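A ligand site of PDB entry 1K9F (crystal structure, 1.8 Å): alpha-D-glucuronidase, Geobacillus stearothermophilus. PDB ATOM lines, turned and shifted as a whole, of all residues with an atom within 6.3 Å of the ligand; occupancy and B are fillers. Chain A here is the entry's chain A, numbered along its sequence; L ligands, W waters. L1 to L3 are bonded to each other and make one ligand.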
ATOM      1  N   TRP A 150      -0.220 -22.065 -32.340  1.00  0.00           N
ATOM      2  CA  TRP A 150       0.177 -21.895 -30.946  1.00  0.00           C
ATOM      3  C   TRP A 150       1.413 -22.765 -30.685  1.00  0.00           C
ATOM      4  O   TRP A 150       1.703 -23.151 -29.555  1.00  0.00           O
ATOM      5  CB  TRP A 150      -0.979 -22.267 -30.004  1.00  0.00           C
ATOM      6  CG  TRP A 150      -2.047 -21.188 -29.966  1.00  0.00           C
ATOM      7  CD1 TRP A 150      -2.065 -20.026 -30.676  1.00  0.00           C
ATOM      8  CD2 TRP A 150      -3.239 -21.171 -29.155  1.00  0.00           C
ATOM      9  NE1 TRP A 150      -3.190 -19.287 -30.371  1.00  0.00           N
ATOM     10  CE2 TRP A 150      -3.923 -19.968 -29.434  1.00  0.00           C
ATOM     11  CE3 TRP A 150      -3.784 -22.060 -28.214  1.00  0.00           C
ATOM     12  CZ2 TRP A 150      -5.130 -19.629 -28.813  1.00  0.00           C
ATOM     13  CZ3 TRP A 150      -4.986 -21.728 -27.597  1.00  0.00           C
ATOM     14  CH2 TRP A 150      -5.652 -20.522 -27.907  1.00  0.00           C
ATOM     15  N   GLU A 158       0.903 -25.399 -27.702  1.00  0.00           N
ATOM     16  CA  GLU A 158      -0.014 -25.126 -26.614  1.00  0.00           C
ATOM     17  C   GLU A 158      -1.422 -25.473 -27.089  1.00  0.00           C
ATOM     18  O   GLU A 158      -1.877 -24.968 -28.120  1.00  0.00           O
ATOM     19  CB  GLU A 158       0.073 -23.654 -26.179  1.00  0.00           C
ATOM     20  CG  GLU A 158      -0.771 -23.352 -24.966  1.00  0.00           C
ATOM     21  CD  GLU A 158      -0.368 -22.065 -24.265  1.00  0.00           C
ATOM     22  OE1 GLU A 158       0.747 -21.557 -24.533  1.00  0.00           O
ATOM     23  OE2 GLU A 158      -1.159 -21.570 -23.432  1.00  0.00           O
ATOM     24  N   ARG A 159      -2.088 -26.340 -26.345  1.00  0.00           N
ATOM     25  CA  ARG A 159      -3.441 -26.808 -26.681  1.00  0.00           C
ATOM     26  C   ARG A 159      -3.394 -27.555 -28.018  1.00  0.00           C
ATOM     27  O   ARG A 159      -4.327 -27.469 -28.819  1.00  0.00           O
ATOM     28  CB  ARG A 159      -4.422 -25.637 -26.762  1.00  0.00           C
ATOM     29  CG  ARG A 159      -4.414 -24.726 -25.544  1.00  0.00           C
ATOM     30  CD  ARG A 159      -4.574 -25.505 -24.238  1.00  0.00           C
ATOM     31  NE  ARG A 159      -4.495 -24.598 -23.086  1.00  0.00           N
ATOM     32  CZ  ARG A 159      -4.601 -24.986 -21.819  1.00  0.00           C
ATOM     33  NH1 ARG A 159      -4.785 -26.261 -21.515  1.00  0.00           N
ATOM     34  NH2 ARG A 159      -4.534 -24.070 -20.848  1.00  0.00           N
ATOM     35  N   ASN A 199       3.321 -19.401 -31.349  1.00  0.00           N
ATOM     36  CA  ASN A 199       2.423 -19.189 -30.220  1.00  0.00           C
ATOM     37  C   ASN A 199       2.220 -17.714 -29.841  1.00  0.00           C
ATOM     38  O   ASN A 199       3.186 -16.943 -29.793  1.00  0.00           O
ATOM     39  CB  ASN A 199       2.978 -19.948 -29.018  1.00  0.00           C
ATOM     40  CG  ASN A 199       1.959 -20.155 -27.912  1.00  0.00           C
ATOM     41  OD1 ASN A 199       0.889 -19.542 -27.910  1.00  0.00           O
ATOM     42  ND2 ASN A 199       2.291 -21.010 -26.960  1.00  0.00           N
ATOM     43  N   VAL A 200       0.973 -17.337 -29.562  1.00  0.00           N
ATOM     44  CA  VAL A 200       0.678 -15.967 -29.163  1.00  0.00           C
ATOM     45  C   VAL A 200       1.346 -15.713 -27.807  1.00  0.00           C
ATOM     46  O   VAL A 200       1.597 -14.562 -27.436  1.00  0.00           O
ATOM     47  CB  VAL A 200      -0.834 -15.717 -29.086  1.00  0.00           C
ATOM     48  CG1 VAL A 200      -1.437 -15.821 -30.489  1.00  0.00           C
ATOM     49  CG2 VAL A 200      -1.501 -16.720 -28.158  1.00  0.00           C
ATOM     50  N   ASN A 201       1.608 -16.783 -27.056  1.00  0.00           N
ATOM     51  CA  ASN A 201       2.313 -16.665 -25.786  1.00  0.00           C
ATOM     52  C   ASN A 201       3.768 -16.838 -26.226  1.00  0.00           C
ATOM     53  O   ASN A 201       4.253 -17.971 -26.346  1.00  0.00           O
ATOM     54  CB  ASN A 201       1.948 -17.784 -24.809  1.00  0.00           C
ATOM     55  CG  ASN A 201       0.578 -17.588 -24.184  1.00  0.00           C
ATOM     56  OD1 ASN A 201       0.212 -16.483 -23.802  1.00  0.00           O
ATOM     57  ND2 ASN A 201      -0.177 -18.680 -24.075  1.00  0.00           N
ATOM     58  N   LYS A 281      -0.436 -10.444 -28.153  1.00  0.00           N
ATOM     59  CA  LYS A 281      -1.168 -10.765 -26.946  1.00  0.00           C
ATOM     60  C   LYS A 281      -0.434  -9.971 -25.873  1.00  0.00           C
ATOM     61  O   LYS A 281       0.676 -10.329 -25.468  1.00  0.00           O
ATOM     62  CB  LYS A 281      -1.112 -12.259 -26.609  1.00  0.00           C
ATOM     63  CG  LYS A 281      -1.788 -12.598 -25.297  1.00  0.00           C
ATOM     64  CD  LYS A 281      -1.747 -14.083 -24.975  1.00  0.00           C
ATOM     65  CE  LYS A 281      -2.304 -14.356 -23.589  1.00  0.00           C
ATOM     66  NZ  LYS A 281      -2.287 -15.813 -23.252  1.00  0.00           N
ATOM     67  N   ARG A 318      -5.026  -8.861 -30.108  1.00  0.00           N
ATOM     68  CA  ARG A 318      -6.027  -9.717 -29.486  1.00  0.00           C
ATOM     69  C   ARG A 318      -6.732  -9.012 -28.328  1.00  0.00           C
ATOM     70  O   ARG A 318      -6.080  -8.409 -27.470  1.00  0.00           O
ATOM     71  CB  ARG A 318      -5.378 -11.015 -28.991  1.00  0.00           C
ATOM     72  CG  ARG A 318      -4.812 -11.860 -30.112  1.00  0.00           C
ATOM     73  CD  ARG A 318      -4.233 -13.166 -29.585  1.00  0.00           C
ATOM     74  NE  ARG A 318      -5.249 -14.183 -29.316  1.00  0.00           N
ATOM     75  CZ  ARG A 318      -5.324 -14.873 -28.183  1.00  0.00           C
ATOM     76  NH1 ARG A 318      -4.464 -14.645 -27.205  1.00  0.00           N
ATOM     77  NH2 ARG A 318      -6.248 -15.819 -28.037  1.00  0.00           N
ATOM     78  N   PHE A 320      -8.422 -10.469 -26.063  1.00  0.00           N
ATOM     79  CA  PHE A 320      -8.608 -11.427 -24.985  1.00  0.00           C
ATOM     80  C   PHE A 320      -7.927 -10.843 -23.755  1.00  0.00           C
ATOM     81  O   PHE A 320      -6.854 -11.293 -23.343  1.00  0.00           O
ATOM     82  CB  PHE A 320      -7.984 -12.772 -25.344  1.00  0.00           C
ATOM     83  CG  PHE A 320      -8.338 -13.882 -24.393  1.00  0.00           C
ATOM     84  CD1 PHE A 320      -9.656 -14.319 -24.279  1.00  0.00           C
ATOM     85  CD2 PHE A 320      -7.359 -14.508 -23.625  1.00  0.00           C
ATOM     86  CE1 PHE A 320     -10.001 -15.352 -23.412  1.00  0.00           C
ATOM     87  CE2 PHE A 320      -7.694 -15.548 -22.752  1.00  0.00           C
ATOM     88  CZ  PHE A 320      -9.016 -15.970 -22.646  1.00  0.00           C
ATOM     89  N   TYR A 322      -8.695  -9.495 -19.696  1.00  0.00           N
ATOM     90  CA  TYR A 322      -9.602  -9.483 -18.551  1.00  0.00           C
ATOM     91  C   TYR A 322      -8.789  -9.606 -17.267  1.00  0.00           C
ATOM     92  O   TYR A 322      -7.568  -9.733 -17.298  1.00  0.00           O
ATOM     93  CB  TYR A 322     -10.582 -10.655 -18.645  1.00  0.00           C
ATOM     94  CG  TYR A 322      -9.906 -12.004 -18.654  1.00  0.00           C
ATOM     95  CD1 TYR A 322      -9.273 -12.480 -19.799  1.00  0.00           C
ATOM     96  CD2 TYR A 322      -9.855 -12.794 -17.500  1.00  0.00           C
ATOM     97  CE1 TYR A 322      -8.613 -13.715 -19.810  1.00  0.00           C
ATOM     98  CE2 TYR A 322      -9.205 -14.029 -17.496  1.00  0.00           C
ATOM     99  CZ  TYR A 322      -8.585 -14.482 -18.655  1.00  0.00           C
ATOM    100  OH  TYR A 322      -7.944 -15.696 -18.656  1.00  0.00           O
ATOM    101  N   ARG A 335     -16.283 -11.278 -15.840  1.00  0.00           N
ATOM    102  CA  ARG A 335     -15.271 -11.439 -16.872  1.00  0.00           C
ATOM    103  C   ARG A 335     -15.857 -11.259 -18.275  1.00  0.00           C
ATOM    104  O   ARG A 335     -15.188 -10.748 -19.179  1.00  0.00           O
ATOM    105  CB  ARG A 335     -14.604 -12.820 -16.747  1.00  0.00           C
ATOM    106  CG  ARG A 335     -13.701 -13.178 -17.915  1.00  0.00           C
ATOM    107  CD  ARG A 335     -12.994 -14.500 -17.669  1.00  0.00           C
ATOM    108  NE  ARG A 335     -12.294 -14.969 -18.856  1.00  0.00           N
ATOM    109  CZ  ARG A 335     -11.516 -16.036 -18.881  1.00  0.00           C
ATOM    110  NH1 ARG A 335     -11.321 -16.756 -17.787  1.00  0.00           N
ATOM    111  NH2 ARG A 335     -10.914 -16.392 -20.011  1.00  0.00           N
ATOM    112  N   LYS A 359     -12.397 -13.135 -29.805  1.00  0.00           N
ATOM    113  CA  LYS A 359     -12.894 -14.510 -29.843  1.00  0.00           C
ATOM    114  C   LYS A 359     -14.392 -14.493 -30.128  1.00  0.00           C
ATOM    115  O   LYS A 359     -15.062 -13.487 -29.849  1.00  0.00           O
ATOM    116  CB  LYS A 359     -12.607 -15.225 -28.514  1.00  0.00           C
ATOM    117  CG  LYS A 359     -11.127 -15.445 -28.252  1.00  0.00           C
ATOM    118  CD  LYS A 359     -10.865 -16.299 -27.026  1.00  0.00           C
ATOM    119  CE  LYS A 359      -9.371 -16.562 -26.853  1.00  0.00           C
ATOM    120  NZ  LYS A 359      -9.096 -17.488 -25.717  1.00  0.00           N
ATOM    121  N   MET A 363     -15.940 -15.158 -23.239  1.00  0.00           N
ATOM    122  CA  MET A 363     -15.238 -15.895 -22.191  1.00  0.00           C
ATOM    123  C   MET A 363     -14.006 -16.603 -22.740  1.00  0.00           C
ATOM    124  O   MET A 363     -12.944 -15.995 -22.819  1.00  0.00           O
ATOM    125  CB  MET A 363     -16.192 -16.878 -21.515  1.00  0.00           C
ATOM    126  CG  MET A 363     -17.299 -16.198 -20.695  1.00  0.00           C
ATOM    127  SD  MET A 363     -16.654 -15.214 -19.308  1.00  0.00           S
ATOM    128  CE  MET A 363     -16.367 -16.509 -18.094  1.00  0.00           C
ATOM    129  N   ASP A 364     -14.129 -17.871 -23.136  1.00  0.00           N
ATOM    130  CA  ASP A 364     -12.959 -18.572 -23.667  1.00  0.00           C
ATOM    131  C   ASP A 364     -13.227 -19.866 -24.431  1.00  0.00           C
ATOM    132  O   ASP A 364     -13.000 -20.964 -23.910  1.00  0.00           O
ATOM    133  CB  ASP A 364     -11.955 -18.831 -22.541  1.00  0.00           C
ATOM    134  CG  ASP A 364     -10.681 -19.532 -23.031  1.00  0.00           C
ATOM    135  OD1 ASP A 364     -10.332 -19.381 -24.224  1.00  0.00           O
ATOM    136  OD2 ASP A 364     -10.034 -20.219 -22.206  1.00  0.00           O
ATOM    137  N   PHE A 365     -13.722 -19.727 -25.648  1.00  0.00           N
ATOM    138  CA  PHE A 365     -13.978 -20.870 -26.524  1.00  0.00           C
ATOM    139  C   PHE A 365     -14.722 -22.057 -25.899  1.00  0.00           C
ATOM    140  O   PHE A 365     -14.379 -23.206 -26.176  1.00  0.00           O
ATOM    141  CB  PHE A 365     -12.655 -21.403 -27.095  1.00  0.00           C
ATOM    142  CG  PHE A 365     -11.872 -20.395 -27.889  1.00  0.00           C
ATOM    143  CD1 PHE A 365     -12.491 -19.632 -28.874  1.00  0.00           C
ATOM    144  CD2 PHE A 365     -10.496 -20.276 -27.721  1.00  0.00           C
ATOM    145  CE1 PHE A 365     -11.741 -18.770 -29.689  1.00  0.00           C
ATOM    146  CE2 PHE A 365      -9.738 -19.416 -28.519  1.00  0.00           C
ATOM    147  CZ  PHE A 365     -10.368 -18.673 -29.511  1.00  0.00           C
ATOM    148  N   GLU A 386     -11.791 -14.424 -33.894  1.00  0.00           N
ATOM    149  CA  GLU A 386     -10.875 -15.540 -33.668  1.00  0.00           C
ATOM    150  C   GLU A 386     -11.701 -16.731 -33.205  1.00  0.00           C
ATOM    151  O   GLU A 386     -12.476 -16.615 -32.265  1.00  0.00           O
ATOM    152  CB  GLU A 386      -9.863 -15.179 -32.580  1.00  0.00           C
ATOM    153  CG  GLU A 386      -8.818 -16.276 -32.310  1.00  0.00           C
ATOM    154  CD  GLU A 386      -7.898 -15.945 -31.150  1.00  0.00           C
ATOM    155  OE1 GLU A 386      -7.562 -14.753 -30.969  1.00  0.00           O
ATOM    156  OE2 GLU A 386      -7.493 -16.876 -30.428  1.00  0.00           O
ATOM    157  N   GLN A 388     -11.526 -21.153 -32.500  1.00  0.00           N
ATOM    158  CA  GLN A 388     -10.538 -22.155 -32.151  1.00  0.00           C
ATOM    159  C   GLN A 388     -10.784 -23.477 -32.851  1.00  0.00           C
ATOM    160  O   GLN A 388     -11.742 -24.180 -32.542  1.00  0.00           O
ATOM    161  CB  GLN A 388     -10.516 -22.336 -30.623  1.00  0.00           C
ATOM    162  CG  GLN A 388      -9.317 -23.113 -30.103  1.00  0.00           C
ATOM    163  CD  GLN A 388      -9.343 -23.269 -28.595  1.00  0.00           C
ATOM    164  OE1 GLN A 388     -10.351 -23.660 -28.009  1.00  0.00           O
ATOM    165  NE2 GLN A 388      -8.213 -22.973 -27.964  1.00  0.00           N
ATOM    166  N   GLU A 392      -9.813 -27.381 -27.706  1.00  0.00           N
ATOM    167  CA  GLU A 392      -9.450 -27.260 -26.302  1.00  0.00           C
ATOM    168  C   GLU A 392     -10.558 -27.644 -25.339  1.00  0.00           C
ATOM    169  O   GLU A 392     -10.356 -28.481 -24.448  1.00  0.00           O
ATOM    170  CB  GLU A 392      -8.976 -25.838 -25.972  1.00  0.00           C
ATOM    171  CG  GLU A 392      -8.586 -25.667 -24.509  1.00  0.00           C
ATOM    172  CD  GLU A 392      -7.967 -24.312 -24.219  1.00  0.00           C
ATOM    173  OE1 GLU A 392      -7.839 -23.492 -25.153  1.00  0.00           O
ATOM    174  OE2 GLU A 392      -7.614 -24.072 -23.041  1.00  0.00           O
ATOM    175  N   TYR A 393     -11.730 -27.041 -25.491  1.00  0.00           N
ATOM    176  CA  TYR A 393     -12.856 -27.324 -24.619  1.00  0.00           C
ATOM    177  C   TYR A 393     -13.928 -28.133 -25.341  1.00  0.00           C
ATOM    178  O   TYR A 393     -15.005 -28.360 -24.806  1.00  0.00           O
ATOM    179  CB  TYR A 393     -13.475 -26.020 -24.112  1.00  0.00           C
ATOM    180  CG  TYR A 393     -12.510 -25.147 -23.335  1.00  0.00           C
ATOM    181  CD1 TYR A 393     -12.192 -25.437 -22.008  1.00  0.00           C
ATOM    182  CD2 TYR A 393     -11.958 -24.005 -23.920  1.00  0.00           C
ATOM    183  CE1 TYR A 393     -11.327 -24.612 -21.279  1.00  0.00           C
ATOM    184  CE2 TYR A 393     -11.097 -23.179 -23.200  1.00  0.00           C
ATOM    185  CZ  TYR A 393     -10.797 -23.482 -21.878  1.00  0.00           C
ATOM    186  OH  TYR A 393      -9.949 -22.657 -21.152  1.00  0.00           O
ATOM    187  N   TRP A 520     -17.658 -24.260 -19.023  1.00  0.00           N
ATOM    188  CA  TRP A 520     -16.660 -24.827 -18.113  1.00  0.00           C
ATOM    189  C   TRP A 520     -16.965 -26.212 -17.545  1.00  0.00           C
ATOM    190  O   TRP A 520     -17.285 -27.122 -18.289  1.00  0.00           O
ATOM    191  CB  TRP A 520     -16.360 -23.805 -17.006  1.00  0.00           C
ATOM    192  CG  TRP A 520     -16.034 -22.467 -17.611  1.00  0.00           C
ATOM    193  CD1 TRP A 520     -16.918 -21.466 -17.920  1.00  0.00           C
ATOM    194  CD2 TRP A 520     -14.778 -22.061 -18.165  1.00  0.00           C
ATOM    195  NE1 TRP A 520     -16.282 -20.473 -18.626  1.00  0.00           N
ATOM    196  CE2 TRP A 520     -14.976 -20.813 -18.794  1.00  0.00           C
ATOM    197  CE3 TRP A 520     -13.494 -22.646 -18.194  1.00  0.00           C
ATOM    198  CZ2 TRP A 520     -13.937 -20.133 -19.452  1.00  0.00           C
ATOM    199  CZ3 TRP A 520     -12.468 -21.966 -18.846  1.00  0.00           C
ATOM    200  CH2 TRP A 520     -12.692 -20.717 -19.463  1.00  0.00           C
ATOM    201  N   PRO A 524      -9.131 -28.397 -14.307  1.00  0.00           N
ATOM    202  CA  PRO A 524      -8.249 -27.236 -14.445  1.00  0.00           C
ATOM    203  C   PRO A 524      -6.930 -27.626 -15.111  1.00  0.00           C
ATOM    204  O   PRO A 524      -6.522 -28.790 -15.077  1.00  0.00           O
ATOM    205  CB  PRO A 524      -8.039 -26.786 -13.003  1.00  0.00           C
ATOM    206  CG  PRO A 524      -9.291 -27.247 -12.302  1.00  0.00           C
ATOM    207  CD  PRO A 524      -9.496 -28.616 -12.893  1.00  0.00           C
ATOM    208  N   GLY A 525      -6.276 -26.649 -15.727  1.00  0.00           N
ATOM    209  CA  GLY A 525      -5.007 -26.925 -16.369  1.00  0.00           C
ATOM    210  C   GLY A 525      -5.104 -27.461 -17.784  1.00  0.00           C
ATOM    211  O   GLY A 525      -5.036 -26.687 -18.728  1.00  0.00           O
ATOM    212  N   HIS A 526      -5.249 -28.779 -17.921  1.00  0.00           N
ATOM    213  CA  HIS A 526      -5.337 -29.379 -19.248  1.00  0.00           C
ATOM    214  C   HIS A 526      -6.720 -29.237 -19.893  1.00  0.00           C
ATOM    215  O   HIS A 526      -6.879 -29.441 -21.089  1.00  0.00           O
ATOM    216  CB  HIS A 526      -4.921 -30.857 -19.195  1.00  0.00           C
ATOM    217  CG  HIS A 526      -5.800 -31.710 -18.341  1.00  0.00           C
ATOM    218  ND1 HIS A 526      -5.417 -32.179 -17.107  1.00  0.00           N
ATOM    219  CD2 HIS A 526      -7.040 -32.206 -18.566  1.00  0.00           C
ATOM    220  CE1 HIS A 526      -6.378 -32.928 -16.603  1.00  0.00           C
ATOM    221  NE2 HIS A 526      -7.372 -32.961 -17.466  1.00  0.00           N
ATOM    222  N   HIS A 527      -7.716 -28.895 -19.081  1.00  0.00           N
ATOM    223  CA  HIS A 527      -9.079 -28.641 -19.547  1.00  0.00           C
ATOM    224  C   HIS A 527      -9.854 -29.782 -20.196  1.00  0.00           C
ATOM    225  O   HIS A 527     -10.855 -29.546 -20.874  1.00  0.00           O
ATOM    226  CB  HIS A 527      -9.048 -27.452 -20.508  1.00  0.00           C
ATOM    227  CG  HIS A 527      -8.558 -26.185 -19.871  1.00  0.00           C
ATOM    228  ND1 HIS A 527      -8.111 -25.104 -20.602  1.00  0.00           N
ATOM    229  CD2 HIS A 527      -8.451 -25.839 -18.569  1.00  0.00           C
ATOM    230  CE1 HIS A 527      -7.745 -24.139 -19.774  1.00  0.00           C
ATOM    231  NE2 HIS A 527      -7.948 -24.556 -18.532  1.00  0.00           N
ATOM    232  N   TYR A 535     -12.952 -24.841 -11.636  1.00  0.00           N
ATOM    233  CA  TYR A 535     -12.530 -23.449 -11.507  1.00  0.00           C
ATOM    234  C   TYR A 535     -13.535 -22.621 -10.718  1.00  0.00           C
ATOM    235  O   TYR A 535     -13.435 -21.393 -10.679  1.00  0.00           O
ATOM    236  CB  TYR A 535     -12.374 -22.825 -12.904  1.00  0.00           C
ATOM    237  CG  TYR A 535     -11.124 -23.210 -13.671  1.00  0.00           C
ATOM    238  CD1 TYR A 535      -9.858 -22.848 -13.217  1.00  0.00           C
ATOM    239  CD2 TYR A 535     -11.214 -23.898 -14.883  1.00  0.00           C
ATOM    240  CE1 TYR A 535      -8.718 -23.154 -13.936  1.00  0.00           C
ATOM    241  CE2 TYR A 535     -10.073 -24.211 -15.614  1.00  0.00           C
ATOM    242  CZ  TYR A 535      -8.828 -23.836 -15.139  1.00  0.00           C
ATOM    243  OH  TYR A 535      -7.693 -24.121 -15.853  1.00  0.00           O
ATOM    244  N   TRP A 540     -10.173 -17.051 -11.992  1.00  0.00           N
ATOM    245  CA  TRP A 540     -10.346 -16.850 -13.427  1.00  0.00           C
ATOM    246  C   TRP A 540     -11.691 -16.273 -13.856  1.00  0.00           C
ATOM    247  O   TRP A 540     -11.916 -16.056 -15.045  1.00  0.00           O
ATOM    248  CB  TRP A 540     -10.091 -18.145 -14.187  1.00  0.00           C
ATOM    249  CG  TRP A 540      -8.680 -18.640 -14.088  1.00  0.00           C
ATOM    250  CD1 TRP A 540      -8.212 -19.631 -13.279  1.00  0.00           C
ATOM    251  CD2 TRP A 540      -7.548 -18.162 -14.832  1.00  0.00           C
ATOM    252  NE1 TRP A 540      -6.862 -19.806 -13.473  1.00  0.00           N
ATOM    253  CE2 TRP A 540      -6.439 -18.919 -14.424  1.00  0.00           C
ATOM    254  CE3 TRP A 540      -7.378 -17.170 -15.810  1.00  0.00           C
ATOM    255  CZ2 TRP A 540      -5.157 -18.715 -14.955  1.00  0.00           C
ATOM    256  CZ3 TRP A 540      -6.110 -16.966 -16.336  1.00  0.00           C
ATOM    257  CH2 TRP A 540      -5.006 -17.738 -15.905  1.00  0.00           C
ATOM    258  N   THR A 542     -14.653 -17.664 -13.896  1.00  0.00           N
ATOM    259  CA  THR A 542     -15.462 -18.627 -14.621  1.00  0.00           C
ATOM    260  C   THR A 542     -16.263 -19.446 -13.612  1.00  0.00           C
ATOM    261  O   THR A 542     -15.847 -20.541 -13.221  1.00  0.00           O
ATOM    262  CB  THR A 542     -14.566 -19.552 -15.459  1.00  0.00           C
ATOM    263  OG1 THR A 542     -13.650 -20.226 -14.590  1.00  0.00           O
ATOM    264  CG2 THR A 542     -13.778 -18.747 -16.463  1.00  0.00           C
HETATM  265  O1  LIG L   1      -0.150 -20.697 -17.186  1.00  0.00           O
HETATM  266  C1  LIG L   1      -1.198 -20.897 -18.064  1.00  0.00           C
HETATM  267  C2  LIG L   1      -1.987 -22.162 -17.671  1.00  0.00           C
HETATM  268  C3  LIG L   1      -3.214 -22.333 -18.552  1.00  0.00           C
HETATM  269  C4  LIG L   1      -4.034 -21.048 -18.551  1.00  0.00           C
HETATM  270  C5  LIG L   1      -3.157 -19.852 -18.937  1.00  0.00           C
HETATM  271  O2  LIG L   1      -1.144 -23.301 -17.810  1.00  0.00           O
HETATM  272  O3  LIG L   1      -4.014 -23.399 -18.066  1.00  0.00           O
HETATM  273  O4  LIG L   1      -5.141 -21.144 -19.458  1.00  0.00           O
HETATM  274  O5  LIG L   1      -2.052 -19.750 -18.018  1.00  0.00           O
HETATM  275  C1  LG2 L   2      -6.266 -20.511 -18.999  1.00  0.00           C
HETATM  276  C2  LG2 L   2      -7.172 -20.054 -20.149  1.00  0.00           C
HETATM  277  C3  LG2 L   2      -8.260 -19.185 -19.473  1.00  0.00           C
HETATM  278  C4  LG2 L   2      -9.027 -20.058 -18.441  1.00  0.00           C
HETATM  279  C5  LG2 L   2      -8.069 -20.730 -17.447  1.00  0.00           C
HETATM  280  O1  LG2 L   2      -6.392 -19.307 -21.135  1.00  0.00           O
HETATM  281  O2  LG2 L   2      -9.162 -18.667 -20.431  1.00  0.00           O
HETATM  282  O3  LG2 L   2      -9.979 -19.276 -17.725  1.00  0.00           O
HETATM  283  O4  LG2 L   2      -6.996 -21.405 -18.140  1.00  0.00           O
HETATM  284  C1  LG3 L   3      -2.227 -19.483 -25.884  1.00  0.00           C
HETATM  285  C2  LG3 L   3      -6.625 -19.630 -22.476  1.00  0.00           C
HETATM  286  C3  LG3 L   3      -5.939 -20.941 -22.938  1.00  0.00           C
HETATM  287  C4  LG3 L   3      -4.484 -20.480 -23.399  1.00  0.00           C
HETATM  288  C5  LG3 L   3      -4.300 -19.457 -24.415  1.00  0.00           C
HETATM  289  C6  LG3 L   3      -5.401 -18.485 -24.108  1.00  0.00           C
HETATM  290  C7  LG3 L   3      -5.430 -17.288 -24.963  1.00  0.00           C
HETATM  291  O1  LG3 L   3      -6.344 -22.031 -22.116  1.00  0.00           O
HETATM  292  O2  LG3 L   3      -3.979 -21.796 -23.713  1.00  0.00           O
HETATM  293  O3  LG3 L   3      -3.095 -18.854 -24.913  1.00  0.00           O
HETATM  294  O4  LG3 L   3      -6.618 -18.468 -23.285  1.00  0.00           O
HETATM  295  O5  LG3 L   3      -6.508 -17.229 -25.790  1.00  0.00           O
HETATM  296  O6  LG3 L   3      -4.367 -16.453 -24.787  1.00  0.00           O
HETATM  297  O   HOH W   1      -5.262 -23.169 -15.152  1.00  0.00           O
HETATM  298  O   HOH W   2     -11.077 -20.786 -15.879  1.00  0.00           O
HETATM  299  O   HOH W   3      -8.101 -20.712 -25.305  1.00  0.00           O
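Water W2 lies within hydrogen-bond range of O3 of LG2 L2 (2.6 Å) and OG1 of Thr 542 (2.9 Å). Water W1 bridges the side-chain hydroxyl of Tyr 535 (2.7 Å) and an oxygen (O3) of LIG L1 (3.2 Å).
Merely in contact with the ligand: Phe 320, Gly 525, Trp 520, Tyr 322, Tyr 535, Val 200, Trp 540, Asn 199, Tyr 393 and Trp 150. Hydrophobic or aromatic side chains within 4 Å of the ligand: Trp 150, Val 200, Phe 320, Trp 520, His 527, Tyr 535 and Trp 540. Within 4 Å of the ligand: Trp 150, Glu 158, Arg 159, Asn 199, Val 200, Asn 201, Lys 281, Arg 318, Phe 320, Tyr 322, Arg 335, Lys 359, Asp 364, Glu 392, Tyr 393, Trp 520, Gly 525, His 527, Tyr 535 and Trp 540.
An oxygen (O2) of LG2 L2 sits at hydrogen-bond distance from the side-chain carboxylate of Asp 364 (2.5 Å). OE2 of Glu 392 sits at hydrogen-bond distance from O1 of LG3 L3 (2.6 Å). The side-chain amino group (NZ) of Lys 359 lies within salt-bridge range of an oxygen (O5) of LG3 L3, at 2.6 Å. The side-chain amino group of Lys 281 is in salt-bridge range of an oxygen (O6) of LG3 L3 (2.7 Å). NH2 of Arg 318 lies within salt-bridge range of O5 of LG3 L3, 2.7 Å away. OE2 of Glu 158 is in hydrogen-bond range of O2 of LG3 L3, at 2.8 Å. The side-chain amide nitrogen (ND2) of Asn 201 sits close to an oxygen (O3) of LG3 L3 (3.0 Å). NH1 of Arg 335 lies within hydrogen-bond range of O3 of LG2 L2 (2.9 Å). An oxygen (O3) of LIG L1 is in hydrogen-bond range of the guanidinium group (NH2) of Arg 159, at 2.9 Å. An oxygen (O4) of LG2 L2 lies close to a ring nitrogen (NE2) of His 527 (3.3 Å).
OE2 of Glu 392 is in salt-bridge range of NE of Arg 159, 3.2 Å away. NE2 of Gln 388 sits at hydrogen-bond distance from OE1 of Glu 392. NZ of Lys 281 is in hydrogen-bond range of OD1 of Asn 201. The side-chain amide nitrogen (ND2) of Asn 201 lies within hydrogen-bond range of the side-chain carboxylate (OE1) of Glu 158. The side-chain carboxylate (OE1) of Glu 158 is in hydrogen-bond range of the side-chain amide nitrogen (ND2) of Asn 199 (2.9 Å). The backbone NH (N) of Glu 158 is in hydrogen-bond range of the backbone carbonyl oxygen (O) of Trp 150 (3.0 Å). The backbone carbonyl oxygen of Gly 525 sits at hydrogen-bond distance from the guanidinium group of Arg 159 (2.8 Å). ND1 of His 527 sits close to OH of Tyr 393.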
